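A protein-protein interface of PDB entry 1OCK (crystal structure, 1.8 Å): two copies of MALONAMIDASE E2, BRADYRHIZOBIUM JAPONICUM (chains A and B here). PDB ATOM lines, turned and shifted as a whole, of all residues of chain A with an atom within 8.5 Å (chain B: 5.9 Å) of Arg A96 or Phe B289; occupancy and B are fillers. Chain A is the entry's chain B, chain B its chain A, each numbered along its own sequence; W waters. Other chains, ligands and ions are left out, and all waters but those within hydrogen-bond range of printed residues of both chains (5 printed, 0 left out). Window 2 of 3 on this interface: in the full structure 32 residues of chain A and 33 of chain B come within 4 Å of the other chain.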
ATOM      1  N   GLN A  49      19.890  16.458  16.181  1.00  0.00           N
ATOM      2  CA  GLN A  49      18.459  16.560  16.423  1.00  0.00           C
ATOM      3  C   GLN A  49      18.342  16.968  17.889  1.00  0.00           C
ATOM      4  O   GLN A  49      19.290  16.792  18.656  1.00  0.00           O
ATOM      5  CB  GLN A  49      17.756  15.227  16.171  1.00  0.00           C
ATOM      6  CG  GLN A  49      17.781  14.795  14.714  1.00  0.00           C
ATOM      7  CD  GLN A  49      16.724  13.759  14.405  1.00  0.00           C
ATOM      8  OE1 GLN A  49      15.527  14.038  14.490  1.00  0.00           O
ATOM      9  NE2 GLN A  49      17.159  12.555  14.048  1.00  0.00           N
ATOM     10  N   SER A  51      15.950  15.841  20.196  1.00  0.00           N
ATOM     11  CA  SER A  51      15.368  14.858  21.105  1.00  0.00           C
ATOM     12  C   SER A  51      15.636  13.421  20.675  1.00  0.00           C
ATOM     13  O   SER A  51      15.966  13.159  19.520  1.00  0.00           O
ATOM     14  CB  SER A  51      13.855  15.073  21.209  1.00  0.00           C
ATOM     15  OG  SER A  51      13.239  14.897  19.947  1.00  0.00           O
ATOM     16  N   GLY A  52      15.478  12.493  21.614  1.00  0.00           N
ATOM     17  CA  GLY A  52      15.702  11.090  21.317  1.00  0.00           C
ATOM     18  C   GLY A  52      16.972  10.569  21.963  1.00  0.00           C
ATOM     19  O   GLY A  52      17.905  11.336  22.203  1.00  0.00           O
ATOM     20  N   PRO A  53      17.045   9.262  22.250  1.00  0.00           N
ATOM     21  CA  PRO A  53      18.241   8.697  22.876  1.00  0.00           C
ATOM     22  C   PRO A  53      19.506   8.833  22.034  1.00  0.00           C
ATOM     23  O   PRO A  53      20.616   8.756  22.563  1.00  0.00           O
ATOM     24  CB  PRO A  53      17.845   7.239  23.120  1.00  0.00           C
ATOM     25  CG  PRO A  53      16.911   6.952  21.987  1.00  0.00           C
ATOM     26  CD  PRO A  53      16.063   8.209  21.939  1.00  0.00           C
ATOM     27  N   LEU A  54      19.350   9.027  20.726  1.00  0.00           N
ATOM     28  CA  LEU A  54      20.514   9.167  19.854  1.00  0.00           C
ATOM     29  C   LEU A  54      20.762  10.606  19.409  1.00  0.00           C
ATOM     30  O   LEU A  54      21.483  10.849  18.441  1.00  0.00           O
ATOM     31  CB  LEU A  54      20.387   8.258  18.626  1.00  0.00           C
ATOM     32  CG  LEU A  54      20.407   6.752  18.903  1.00  0.00           C
ATOM     33  CD1 LEU A  54      20.413   5.996  17.582  1.00  0.00           C
ATOM     34  CD2 LEU A  54      21.636   6.390  19.725  1.00  0.00           C
ATOM     35  N   ARG A  55      20.168  11.565  20.109  1.00  0.00           N
ATOM     36  CA  ARG A  55      20.387  12.961  19.754  1.00  0.00           C
ATOM     37  C   ARG A  55      21.869  13.268  19.967  1.00  0.00           C
ATOM     38  O   ARG A  55      22.449  12.885  20.982  1.00  0.00           O
ATOM     39  CB  ARG A  55      19.518  13.882  20.619  1.00  0.00           C
ATOM     40  CG  ARG A  55      19.793  13.825  22.118  1.00  0.00           C
ATOM     41  CD  ARG A  55      18.817  14.732  22.864  1.00  0.00           C
ATOM     42  NE  ARG A  55      19.064  14.781  24.303  1.00  0.00           N
ATOM     43  CZ  ARG A  55      18.775  13.802  25.153  1.00  0.00           C
ATOM     44  NH1 ARG A  55      18.223  12.678  24.717  1.00  0.00           N
ATOM     45  NH2 ARG A  55      19.032  13.948  26.449  1.00  0.00           N
ATOM     46  N   PRO A  89      14.528   1.642   5.832  1.00  0.00           N
ATOM     47  CA  PRO A  89      13.952   1.486   7.167  1.00  0.00           C
ATOM     48  C   PRO A  89      14.987   1.513   8.308  1.00  0.00           C
ATOM     49  O   PRO A  89      14.715   2.091   9.360  1.00  0.00           O
ATOM     50  CB  PRO A  89      13.224   0.156   7.058  1.00  0.00           C
ATOM     51  CG  PRO A  89      12.674   0.216   5.671  1.00  0.00           C
ATOM     52  CD  PRO A  89      13.851   0.758   4.863  1.00  0.00           C
ATOM     53  N   VAL A  90      16.162   0.904   8.125  1.00  0.00           N
ATOM     54  CA  VAL A  90      17.155   0.934   9.208  1.00  0.00           C
ATOM     55  C   VAL A  90      17.690   2.342   9.416  1.00  0.00           C
ATOM     56  O   VAL A  90      18.056   2.712  10.532  1.00  0.00           O
ATOM     57  CB  VAL A  90      18.350  -0.033   8.980  1.00  0.00           C
ATOM     58  CG1 VAL A  90      17.878  -1.462   9.136  1.00  0.00           C
ATOM     59  CG2 VAL A  90      18.979   0.191   7.613  1.00  0.00           C
ATOM     60  N   VAL A  91      17.736   3.127   8.343  1.00  0.00           N
ATOM     61  CA  VAL A  91      18.185   4.512   8.438  1.00  0.00           C
ATOM     62  C   VAL A  91      17.123   5.299   9.214  1.00  0.00           C
ATOM     63  O   VAL A  91      17.446   6.138  10.059  1.00  0.00           O
ATOM     64  CB  VAL A  91      18.379   5.140   7.034  1.00  0.00           C
ATOM     65  CG1 VAL A  91      18.553   6.653   7.145  1.00  0.00           C
ATOM     66  CG2 VAL A  91      19.605   4.526   6.362  1.00  0.00           C
ATOM     67  N   MET A  92      15.855   5.014   8.937  1.00  0.00           N
ATOM     68  CA  MET A  92      14.768   5.696   9.634  1.00  0.00           C
ATOM     69  C   MET A  92      14.725   5.304  11.111  1.00  0.00           C
ATOM     70  O   MET A  92      14.324   6.104  11.954  1.00  0.00           O
ATOM     71  CB  MET A  92      13.424   5.389   8.973  1.00  0.00           C
ATOM     72  CG  MET A  92      13.221   6.080   7.642  1.00  0.00           C
ATOM     73  SD  MET A  92      13.378   7.875   7.767  1.00  0.00           S
ATOM     74  CE  MET A  92      12.083   8.260   8.958  1.00  0.00           C
ATOM     75  N   MET A  93      15.125   4.077  11.428  1.00  0.00           N
ATOM     76  CA  MET A  93      15.146   3.643  12.822  1.00  0.00           C
ATOM     77  C   MET A  93      16.132   4.517  13.592  1.00  0.00           C
ATOM     78  O   MET A  93      15.903   4.862  14.750  1.00  0.00           O
ATOM     79  CB  MET A  93      15.572   2.179  12.930  1.00  0.00           C
ATOM     80  CG  MET A  93      14.587   1.194  12.331  1.00  0.00           C
ATOM     81  SD  MET A  93      15.187  -0.507  12.477  1.00  0.00           S
ATOM     82  CE  MET A  93      13.632  -1.416  12.443  1.00  0.00           C
ATOM     83  N   LEU A  94      17.231   4.881  12.942  1.00  0.00           N
ATOM     84  CA  LEU A  94      18.231   5.717  13.588  1.00  0.00           C
ATOM     85  C   LEU A  94      17.749   7.158  13.698  1.00  0.00           C
ATOM     86  O   LEU A  94      17.891   7.791  14.748  1.00  0.00           O
ATOM     87  CB  LEU A  94      19.551   5.670  12.809  1.00  0.00           C
ATOM     88  CG  LEU A  94      20.279   4.317  12.840  1.00  0.00           C
ATOM     89  CD1 LEU A  94      21.338   4.283  11.744  1.00  0.00           C
ATOM     90  CD2 LEU A  94      20.920   4.101  14.210  1.00  0.00           C
ATOM     91  N   LYS A  95      17.163   7.671  12.621  1.00  0.00           N
ATOM     92  CA  LYS A  95      16.684   9.048  12.619  1.00  0.00           C
ATOM     93  C   LYS A  95      15.545   9.286  13.602  1.00  0.00           C
ATOM     94  O   LYS A  95      15.508  10.310  14.276  1.00  0.00           O
ATOM     95  CB  LYS A  95      16.242   9.466  11.214  1.00  0.00           C
ATOM     96  CG  LYS A  95      17.365   9.501  10.185  1.00  0.00           C
ATOM     97  CD  LYS A  95      17.057  10.478   9.056  1.00  0.00           C
ATOM     98  CE  LYS A  95      15.709  10.206   8.415  1.00  0.00           C
ATOM     99  NZ  LYS A  95      15.364  11.212   7.363  1.00  0.00           N
ATOM    100  N   ARG A  96      14.608   8.351  13.683  1.00  0.00           N
ATOM    101  CA  ARG A  96      13.494   8.519  14.605  1.00  0.00           C
ATOM    102  C   ARG A  96      13.959   8.473  16.052  1.00  0.00           C
ATOM    103  O   ARG A  96      13.255   8.931  16.951  1.00  0.00           O
ATOM    104  CB  ARG A  96      12.433   7.454  14.354  1.00  0.00           C
ATOM    105  CG  ARG A  96      11.634   7.701  13.090  1.00  0.00           C
ATOM    106  CD  ARG A  96      10.597   6.624  12.916  1.00  0.00           C
ATOM    107  NE  ARG A  96       9.644   6.938  11.858  1.00  0.00           N
ATOM    108  CZ  ARG A  96       8.503   6.282  11.686  1.00  0.00           C
ATOM    109  NH1 ARG A  96       8.190   5.281  12.501  1.00  0.00           N
ATOM    110  NH2 ARG A  96       7.669   6.636  10.718  1.00  0.00           N
ATOM    111  N   ALA A  97      15.153   7.928  16.270  1.00  0.00           N
ATOM    112  CA  ALA A  97      15.726   7.842  17.607  1.00  0.00           C
ATOM    113  C   ALA A  97      16.504   9.123  17.914  1.00  0.00           C
ATOM    114  O   ALA A  97      17.024   9.295  19.015  1.00  0.00           O
ATOM    115  CB  ALA A  97      16.641   6.621  17.713  1.00  0.00           C
ATOM    116  N   GLY A  98      16.580  10.012  16.924  1.00  0.00           N
ATOM    117  CA  GLY A  98      17.265  11.280  17.101  1.00  0.00           C
ATOM    118  C   GLY A  98      18.675  11.385  16.555  1.00  0.00           C
ATOM    119  O   GLY A  98      19.341  12.397  16.757  1.00  0.00           O
ATOM    120  N   ALA A  99      19.133  10.356  15.854  1.00  0.00           N
ATOM    121  CA  ALA A  99      20.483  10.353  15.303  1.00  0.00           C
ATOM    122  C   ALA A  99      20.677  11.256  14.091  1.00  0.00           C
ATOM    123  O   ALA A  99      19.719  11.668  13.433  1.00  0.00           O
ATOM    124  CB  ALA A  99      20.887   8.920  14.936  1.00  0.00           C
ATOM    125  N   THR A 100      21.939  11.553  13.804  1.00  0.00           N
ATOM    126  CA  THR A 100      22.307  12.369  12.655  1.00  0.00           C
ATOM    127  C   THR A 100      23.047  11.475  11.663  1.00  0.00           C
ATOM    128  O   THR A 100      24.024  10.824  12.027  1.00  0.00           O
ATOM    129  CB  THR A 100      23.246  13.527  13.060  1.00  0.00           C
ATOM    130  OG1 THR A 100      22.575  14.381  13.993  1.00  0.00           O
ATOM    131  CG2 THR A 100      23.659  14.344  11.828  1.00  0.00           C
ATOM    132  N   ILE A 101      22.560  11.415  10.427  1.00  0.00           N
ATOM    133  CA  ILE A 101      23.222  10.623   9.391  1.00  0.00           C
ATOM    134  C   ILE A 101      24.283  11.576   8.855  1.00  0.00           C
ATOM    135  O   ILE A 101      23.979  12.491   8.091  1.00  0.00           O
ATOM    136  CB  ILE A 101      22.238  10.234   8.268  1.00  0.00           C
ATOM    137  CG1 ILE A 101      21.038   9.491   8.861  1.00  0.00           C
ATOM    138  CG2 ILE A 101      22.941   9.372   7.232  1.00  0.00           C
ATOM    139  CD1 ILE A 101      21.401   8.253   9.671  1.00  0.00           C
ATOM    140  N   ALA A 206      18.125   1.690  20.867  1.00  0.00           N
ATOM    141  CA  ALA A 206      17.490   2.866  20.280  1.00  0.00           C
ATOM    142  C   ALA A 206      16.833   2.552  18.939  1.00  0.00           C
ATOM    143  O   ALA A 206      15.801   3.128  18.596  1.00  0.00           O
ATOM    144  CB  ALA A 206      18.513   3.981  20.107  1.00  0.00           C
ATOM    145  N   MET A 207      17.434   1.645  18.178  1.00  0.00           N
ATOM    146  CA  MET A 207      16.894   1.280  16.871  1.00  0.00           C
ATOM    147  C   MET A 207      15.663   0.388  16.954  1.00  0.00           C
ATOM    148  O   MET A 207      14.687   0.601  16.234  1.00  0.00           O
ATOM    149  CB  MET A 207      17.953   0.560  16.025  1.00  0.00           C
ATOM    150  CG  MET A 207      19.095   1.433  15.519  1.00  0.00           C
ATOM    151  SD  MET A 207      20.286   0.473  14.542  1.00  0.00           S
ATOM    152  CE  MET A 207      19.466   0.417  12.955  1.00  0.00           C
ATOM    153  N   HIS B 282       4.856   0.069   9.682  1.00  0.00           N
ATOM    154  CA  HIS B 282       5.374   1.325  10.212  1.00  0.00           C
ATOM    155  C   HIS B 282       6.878   1.450  10.001  1.00  0.00           C
ATOM    156  O   HIS B 282       7.382   2.543   9.740  1.00  0.00           O
ATOM    157  CB  HIS B 282       5.027   1.469  11.698  1.00  0.00           C
ATOM    158  CG  HIS B 282       3.733   2.180  11.934  1.00  0.00           C
ATOM    159  ND1 HIS B 282       3.586   3.533  11.719  1.00  0.00           N
ATOM    160  CD2 HIS B 282       2.508   1.717  12.274  1.00  0.00           C
ATOM    161  CE1 HIS B 282       2.325   3.873  11.915  1.00  0.00           C
ATOM    162  NE2 HIS B 282       1.649   2.788  12.251  1.00  0.00           N
ATOM    163  N   ARG B 283       7.599   0.337  10.114  1.00  0.00           N
ATOM    164  CA  ARG B 283       9.049   0.369   9.901  1.00  0.00           C
ATOM    165  C   ARG B 283       9.361   0.458   8.411  1.00  0.00           C
ATOM    166  O   ARG B 283      10.228   1.222   7.989  1.00  0.00           O
ATOM    167  CB  ARG B 283       9.720  -0.904  10.435  1.00  0.00           C
ATOM    168  CG  ARG B 283      10.168  -0.877  11.885  1.00  0.00           C
ATOM    169  CD  ARG B 283       9.005  -0.831  12.837  1.00  0.00           C
ATOM    170  NE  ARG B 283       8.695   0.531  13.260  1.00  0.00           N
ATOM    171  CZ  ARG B 283       7.600   0.860  13.933  1.00  0.00           C
ATOM    172  NH1 ARG B 283       6.716  -0.073  14.252  1.00  0.00           N
ATOM    173  NH2 ARG B 283       7.387   2.122  14.290  1.00  0.00           N
ATOM    174  N   LEU B 285       7.518   1.613   5.968  1.00  0.00           N
ATOM    175  CA  LEU B 285       7.080   2.863   5.349  1.00  0.00           C
ATOM    176  C   LEU B 285       7.390   4.037   6.278  1.00  0.00           C
ATOM    177  O   LEU B 285       6.702   5.058   6.258  1.00  0.00           O
ATOM    178  CB  LEU B 285       5.568   2.815   5.064  1.00  0.00           C
ATOM    179  CG  LEU B 285       5.080   1.745   4.082  1.00  0.00           C
ATOM    180  CD1 LEU B 285       3.560   1.688   4.093  1.00  0.00           C
ATOM    181  CD2 LEU B 285       5.601   2.048   2.684  1.00  0.00           C
ATOM    182  N   ALA B 286       8.436   3.891   7.085  1.00  0.00           N
ATOM    183  CA  ALA B 286       8.821   4.929   8.037  1.00  0.00           C
ATOM    184  C   ALA B 286       9.126   6.271   7.377  1.00  0.00           C
ATOM    185  O   ALA B 286       8.675   7.314   7.841  1.00  0.00           O
ATOM    186  CB  ALA B 286      10.017   4.470   8.851  1.00  0.00           C
ATOM    187  N   TRP B 287       9.897   6.247   6.298  1.00  0.00           N
ATOM    188  CA  TRP B 287      10.234   7.486   5.612  1.00  0.00           C
ATOM    189  C   TRP B 287       8.972   8.215   5.126  1.00  0.00           C
ATOM    190  O   TRP B 287       8.807   9.419   5.354  1.00  0.00           O
ATOM    191  CB  TRP B 287      11.144   7.194   4.420  1.00  0.00           C
ATOM    192  CG  TRP B 287      11.489   8.419   3.631  1.00  0.00           C
ATOM    193  CD1 TRP B 287      12.413   9.370   3.955  1.00  0.00           C
ATOM    194  CD2 TRP B 287      10.905   8.830   2.390  1.00  0.00           C
ATOM    195  NE1 TRP B 287      12.446  10.346   2.987  1.00  0.00           N
ATOM    196  CE2 TRP B 287      11.531  10.039   2.016  1.00  0.00           C
ATOM    197  CE3 TRP B 287       9.916   8.292   1.554  1.00  0.00           C
ATOM    198  CZ2 TRP B 287      11.198  10.723   0.841  1.00  0.00           C
ATOM    199  CZ3 TRP B 287       9.586   8.973   0.385  1.00  0.00           C
ATOM    200  CH2 TRP B 287      10.230  10.175   0.041  1.00  0.00           C
ATOM    201  N   GLU B 288       8.086   7.485   4.455  1.00  0.00           N
ATOM    202  CA  GLU B 288       6.856   8.081   3.933  1.00  0.00           C
ATOM    203  C   GLU B 288       5.973   8.652   5.047  1.00  0.00           C
ATOM    204  O   GLU B 288       5.427   9.755   4.922  1.00  0.00           O
ATOM    205  CB  GLU B 288       6.054   7.045   3.124  1.00  0.00           C
ATOM    206  CG  GLU B 288       6.693   6.640   1.796  1.00  0.00           C
ATOM    207  CD  GLU B 288       7.700   5.499   1.916  1.00  0.00           C
ATOM    208  OE1 GLU B 288       8.144   5.177   3.042  1.00  0.00           O
ATOM    209  OE2 GLU B 288       8.053   4.930   0.864  1.00  0.00           O
ATOM    210  N   PHE B 289       5.847   7.905   6.139  1.00  0.00           N
ATOM    211  CA  PHE B 289       5.016   8.324   7.265  1.00  0.00           C
ATOM    212  C   PHE B 289       5.601   9.529   8.005  1.00  0.00           C
ATOM    213  O   PHE B 289       4.869  10.422   8.435  1.00  0.00           O
ATOM    214  CB  PHE B 289       4.839   7.151   8.232  1.00  0.00           C
ATOM    215  CG  PHE B 289       3.807   7.389   9.300  1.00  0.00           C
ATOM    216  CD1 PHE B 289       2.450   7.307   9.008  1.00  0.00           C
ATOM    217  CD2 PHE B 289       4.195   7.673  10.603  1.00  0.00           C
ATOM    218  CE1 PHE B 289       1.488   7.501  10.006  1.00  0.00           C
ATOM    219  CE2 PHE B 289       3.246   7.869  11.609  1.00  0.00           C
ATOM    220  CZ  PHE B 289       1.892   7.781  11.309  1.00  0.00           C
ATOM    221  N   SER B 290       6.920   9.562   8.151  1.00  0.00           N
ATOM    222  CA  SER B 290       7.561  10.667   8.857  1.00  0.00           C
ATOM    223  C   SER B 290       7.730  11.925   8.002  1.00  0.00           C
ATOM    224  O   SER B 290       7.562  13.038   8.497  1.00  0.00           O
ATOM    225  CB  SER B 290       8.940  10.244   9.384  1.00  0.00           C
ATOM    226  OG  SER B 290       8.837   9.223  10.363  1.00  0.00           O
ATOM    227  N   GLU B 291       8.039  11.740   6.723  1.00  0.00           N
ATOM    228  CA  GLU B 291       8.301  12.857   5.817  1.00  0.00           C
ATOM    229  C   GLU B 291       7.183  13.274   4.862  1.00  0.00           C
ATOM    230  O   GLU B 291       7.186  14.403   4.369  1.00  0.00           O
ATOM    231  CB  GLU B 291       9.545  12.551   4.978  1.00  0.00           C
ATOM    232  CG  GLU B 291      10.716  11.954   5.742  1.00  0.00           C
ATOM    233  CD  GLU B 291      11.426  12.952   6.629  1.00  0.00           C
ATOM    234  OE1 GLU B 291      12.520  12.613   7.131  1.00  0.00           O
ATOM    235  OE2 GLU B 291      10.901  14.068   6.826  1.00  0.00           O
ATOM    236  N   HIS B 292       6.246  12.373   4.584  1.00  0.00           N
ATOM    237  CA  HIS B 292       5.158  12.677   3.658  1.00  0.00           C
ATOM    238  C   HIS B 292       3.827  12.137   4.156  1.00  0.00           C
ATOM    239  O   HIS B 292       3.005  11.658   3.377  1.00  0.00           O
ATOM    240  CB  HIS B 292       5.490  12.091   2.283  1.00  0.00           C
ATOM    241  CG  HIS B 292       6.751  12.645   1.698  1.00  0.00           C
ATOM    242  ND1 HIS B 292       6.828  13.918   1.175  1.00  0.00           N
ATOM    243  CD2 HIS B 292       8.009  12.145   1.653  1.00  0.00           C
ATOM    244  CE1 HIS B 292       8.079  14.181   0.839  1.00  0.00           C
ATOM    245  NE2 HIS B 292       8.816  13.122   1.122  1.00  0.00           N
ATOM    246  N   HIS B 293       3.622  12.240   5.463  1.00  0.00           N
ATOM    247  CA  HIS B 293       2.415  11.752   6.113  1.00  0.00           C
ATOM    248  C   HIS B 293       1.104  12.128   5.421  1.00  0.00           C
ATOM    249  O   HIS B 293       0.319  11.258   5.052  1.00  0.00           O
ATOM    250  CB  HIS B 293       2.394  12.227   7.569  1.00  0.00           C
ATOM    251  CG  HIS B 293       1.165  11.820   8.320  1.00  0.00           C
ATOM    252  ND1 HIS B 293      -0.030  12.501   8.221  1.00  0.00           N
ATOM    253  CD2 HIS B 293       0.940  10.786   9.165  1.00  0.00           C
ATOM    254  CE1 HIS B 293      -0.938  11.903   8.971  1.00  0.00           C
ATOM    255  NE2 HIS B 293      -0.376  10.860   9.555  1.00  0.00           N
ATOM    256  N   ILE B 296       0.151  10.427   2.064  1.00  0.00           N
ATOM    257  CA  ILE B 296      -0.175   9.010   2.003  1.00  0.00           C
ATOM    258  C   ILE B 296      -1.678   8.892   1.787  1.00  0.00           C
ATOM    259  O   ILE B 296      -2.455   9.603   2.431  1.00  0.00           O
ATOM    260  CB  ILE B 296       0.210   8.292   3.317  1.00  0.00           C
ATOM    261  CG1 ILE B 296       1.735   8.237   3.440  1.00  0.00           C
ATOM    262  CG2 ILE B 296      -0.401   6.897   3.352  1.00  0.00           C
ATOM    263  CD1 ILE B 296       2.243   7.675   4.757  1.00  0.00           C
ATOM    264  N   ARG B 301      -3.185   5.881   5.389  1.00  0.00           N
ATOM    265  CA  ARG B 301      -2.764   6.901   6.341  1.00  0.00           C
ATOM    266  C   ARG B 301      -3.498   6.680   7.660  1.00  0.00           C
ATOM    267  O   ARG B 301      -2.911   6.789   8.732  1.00  0.00           O
ATOM    268  CB  ARG B 301      -3.078   8.300   5.792  1.00  0.00           C
ATOM    269  CG  ARG B 301      -2.400   9.435   6.550  1.00  0.00           C
ATOM    270  CD  ARG B 301      -2.559  10.760   5.810  1.00  0.00           C
ATOM    271  NE  ARG B 301      -3.917  11.280   5.893  1.00  0.00           N
ATOM    272  CZ  ARG B 301      -4.618  11.720   4.851  1.00  0.00           C
ATOM    273  NH1 ARG B 301      -4.096  11.702   3.630  1.00  0.00           N
ATOM    274  NH2 ARG B 301      -5.845  12.183   5.036  1.00  0.00           N
ATOM    275  N   LEU B 304      -2.237   3.469   9.460  1.00  0.00           N
ATOM    276  CA  LEU B 304      -0.928   3.718  10.055  1.00  0.00           C
ATOM    277  C   LEU B 304      -1.128   4.565  11.309  1.00  0.00           C
ATOM    278  O   LEU B 304      -0.586   4.264  12.371  1.00  0.00           O
ATOM    279  CB  LEU B 304      -0.011   4.440   9.056  1.00  0.00           C
ATOM    280  CG  LEU B 304       0.461   3.596   7.861  1.00  0.00           C
ATOM    281  CD1 LEU B 304       1.136   4.475   6.820  1.00  0.00           C
ATOM    282  CD2 LEU B 304       1.427   2.513   8.354  1.00  0.00           C
ATOM    283  N   ASP B 305      -1.932   5.617  11.193  1.00  0.00           N
ATOM    284  CA  ASP B 305      -2.184   6.481  12.339  1.00  0.00           C
ATOM    285  C   ASP B 305      -2.747   5.709  13.526  1.00  0.00           C
ATOM    286  O   ASP B 305      -2.379   5.962  14.669  1.00  0.00           O
ATOM    287  CB  ASP B 305      -3.153   7.607  11.953  1.00  0.00           C
ATOM    288  CG  ASP B 305      -2.474   8.720  11.174  1.00  0.00           C
ATOM    289  OD1 ASP B 305      -3.190   9.561  10.586  1.00  0.00           O
ATOM    290  OD2 ASP B 305      -1.227   8.768  11.157  1.00  0.00           O
ATOM    291  N   VAL B 308       0.230   3.319  15.354  1.00  0.00           N
ATOM    292  CA  VAL B 308       1.535   3.848  15.741  1.00  0.00           C
ATOM    293  C   VAL B 308       2.010   3.309  17.088  1.00  0.00           C
ATOM    294  O   VAL B 308       3.211   3.223  17.340  1.00  0.00           O
ATOM    295  CB  VAL B 308       1.519   5.393  15.823  1.00  0.00           C
ATOM    296  CG1 VAL B 308       1.204   5.988  14.460  1.00  0.00           C
ATOM    297  CG2 VAL B 308       0.499   5.850  16.853  1.00  0.00           C
HETATM  298  O   HOH W   1       9.528   4.094  15.011  1.00  0.00           O
HETATM  299  O   HOH W   2       5.348   5.095  13.456  1.00  0.00           O
HETATM  300  O   HOH W   3      12.511  11.563   9.337  1.00  0.00           O
HETATM  301  O   HOH W   4       5.829   4.747  10.142  1.00  0.00           O
HETATM  302  O   HOH W   5      12.022   1.845  10.159  1.00  0.00           O
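Val A91 touches none of the printed residues of chain B. Of the printed residues of chain B, Met A93 touches Arg B283 (3.5 Å). Arg A96 touches five residues of chain B. Gly A98 touches none of the printed residues of chain B. Of the printed residues of chain A, Trp B287 touches Met A92. Ser B290 touches just these residues of chain A: Met A92 and Arg A96. The nearest residue of chain B that does not touch Arg A96 is Leu B285 (4.8 Å). The nearest residue of chain A that does not touch Phe B289 is Met A92 (6.7 Å). The nearest printed residue of chain A that does not touch His B282 is Met A92 (6.7 Å).
No position is printed for both chains. Of the 11 pairs that touch across the chains among the printed residues, none has its exchanged pair printed and touching as well.
A ring nitrogen (NE2) of His B282 lies within hydrogen-bond range of the backbone carbonyl oxygen of Leu B304, at 2.7 Å. N of Val B308 sits at hydrogen-bond distance from NE2 of His B282 (3.5 Å). O of Ala B286 sits at hydrogen-bond distance from OG of Ser B290 (3.2 Å). The side-chain amide nitrogen of Gln A49 lies within hydrogen-bond range of the backbone carbonyl oxygen of Lys A95 (2.8 Å).
Among the printed residues, merely in contact across the chains: Pro A89 with Arg B283, Met A92 with Ala B286, Met A93 with Arg B283, Met A92 with Trp B287, Arg A96 with Phe B289, Met A92 with Ser B290, Arg A96 with Arg B283 and Arg A96 with His B282.
Of the 16 printed residues of chain B, 7 touch a printed residue of chain A. Of the 21 printed residues of chain A, 5 touch a printed residue of chain B. Hydrophobic or aromatic side chains of chain A within 4 Å of the printed part of chain B: Pro A89, Met A92 and Met A93. Among the printed residues, Asp or Glu carboxylates within 4 Å of a Lys or Arg side-chain nitrogen of the other chain: Lys A95 with Glu B291 (3.2 Å).
Water W3 bridges the side-chain carboxylate of Glu B291 (2.4 Å) and the side-chain amino group of Lys A95 (3.5 Å). Water W4 bridges the guanidinium group (NH2) of Arg A96 (2.7 Å) and the backbone carbonyl oxygen (O) of His B282 (2.7 Å). Water W5 bridges the backbone carbonyl oxygen (O) of Pro A89 (2.8 Å) and the backbone carbonyl oxygen (O) of Arg B283 (2.9 Å). Water W2 bridges ND1 of His B282 and NH1 of Arg A96. Water W1 bridges NH2 of Arg B283 and NH1 of Arg A96.
NH2 of Arg A96 sits at hydrogen-bond distance from O of Ala B286 (3.1 Å). The guanidinium group (NE) of Arg A96 is in hydrogen-bond range of the side-chain hydroxyl (OG) of Ser B290, 2.8 Å away. OE1 of Glu B291 lies within salt-bridge range of NZ of Lys A95.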
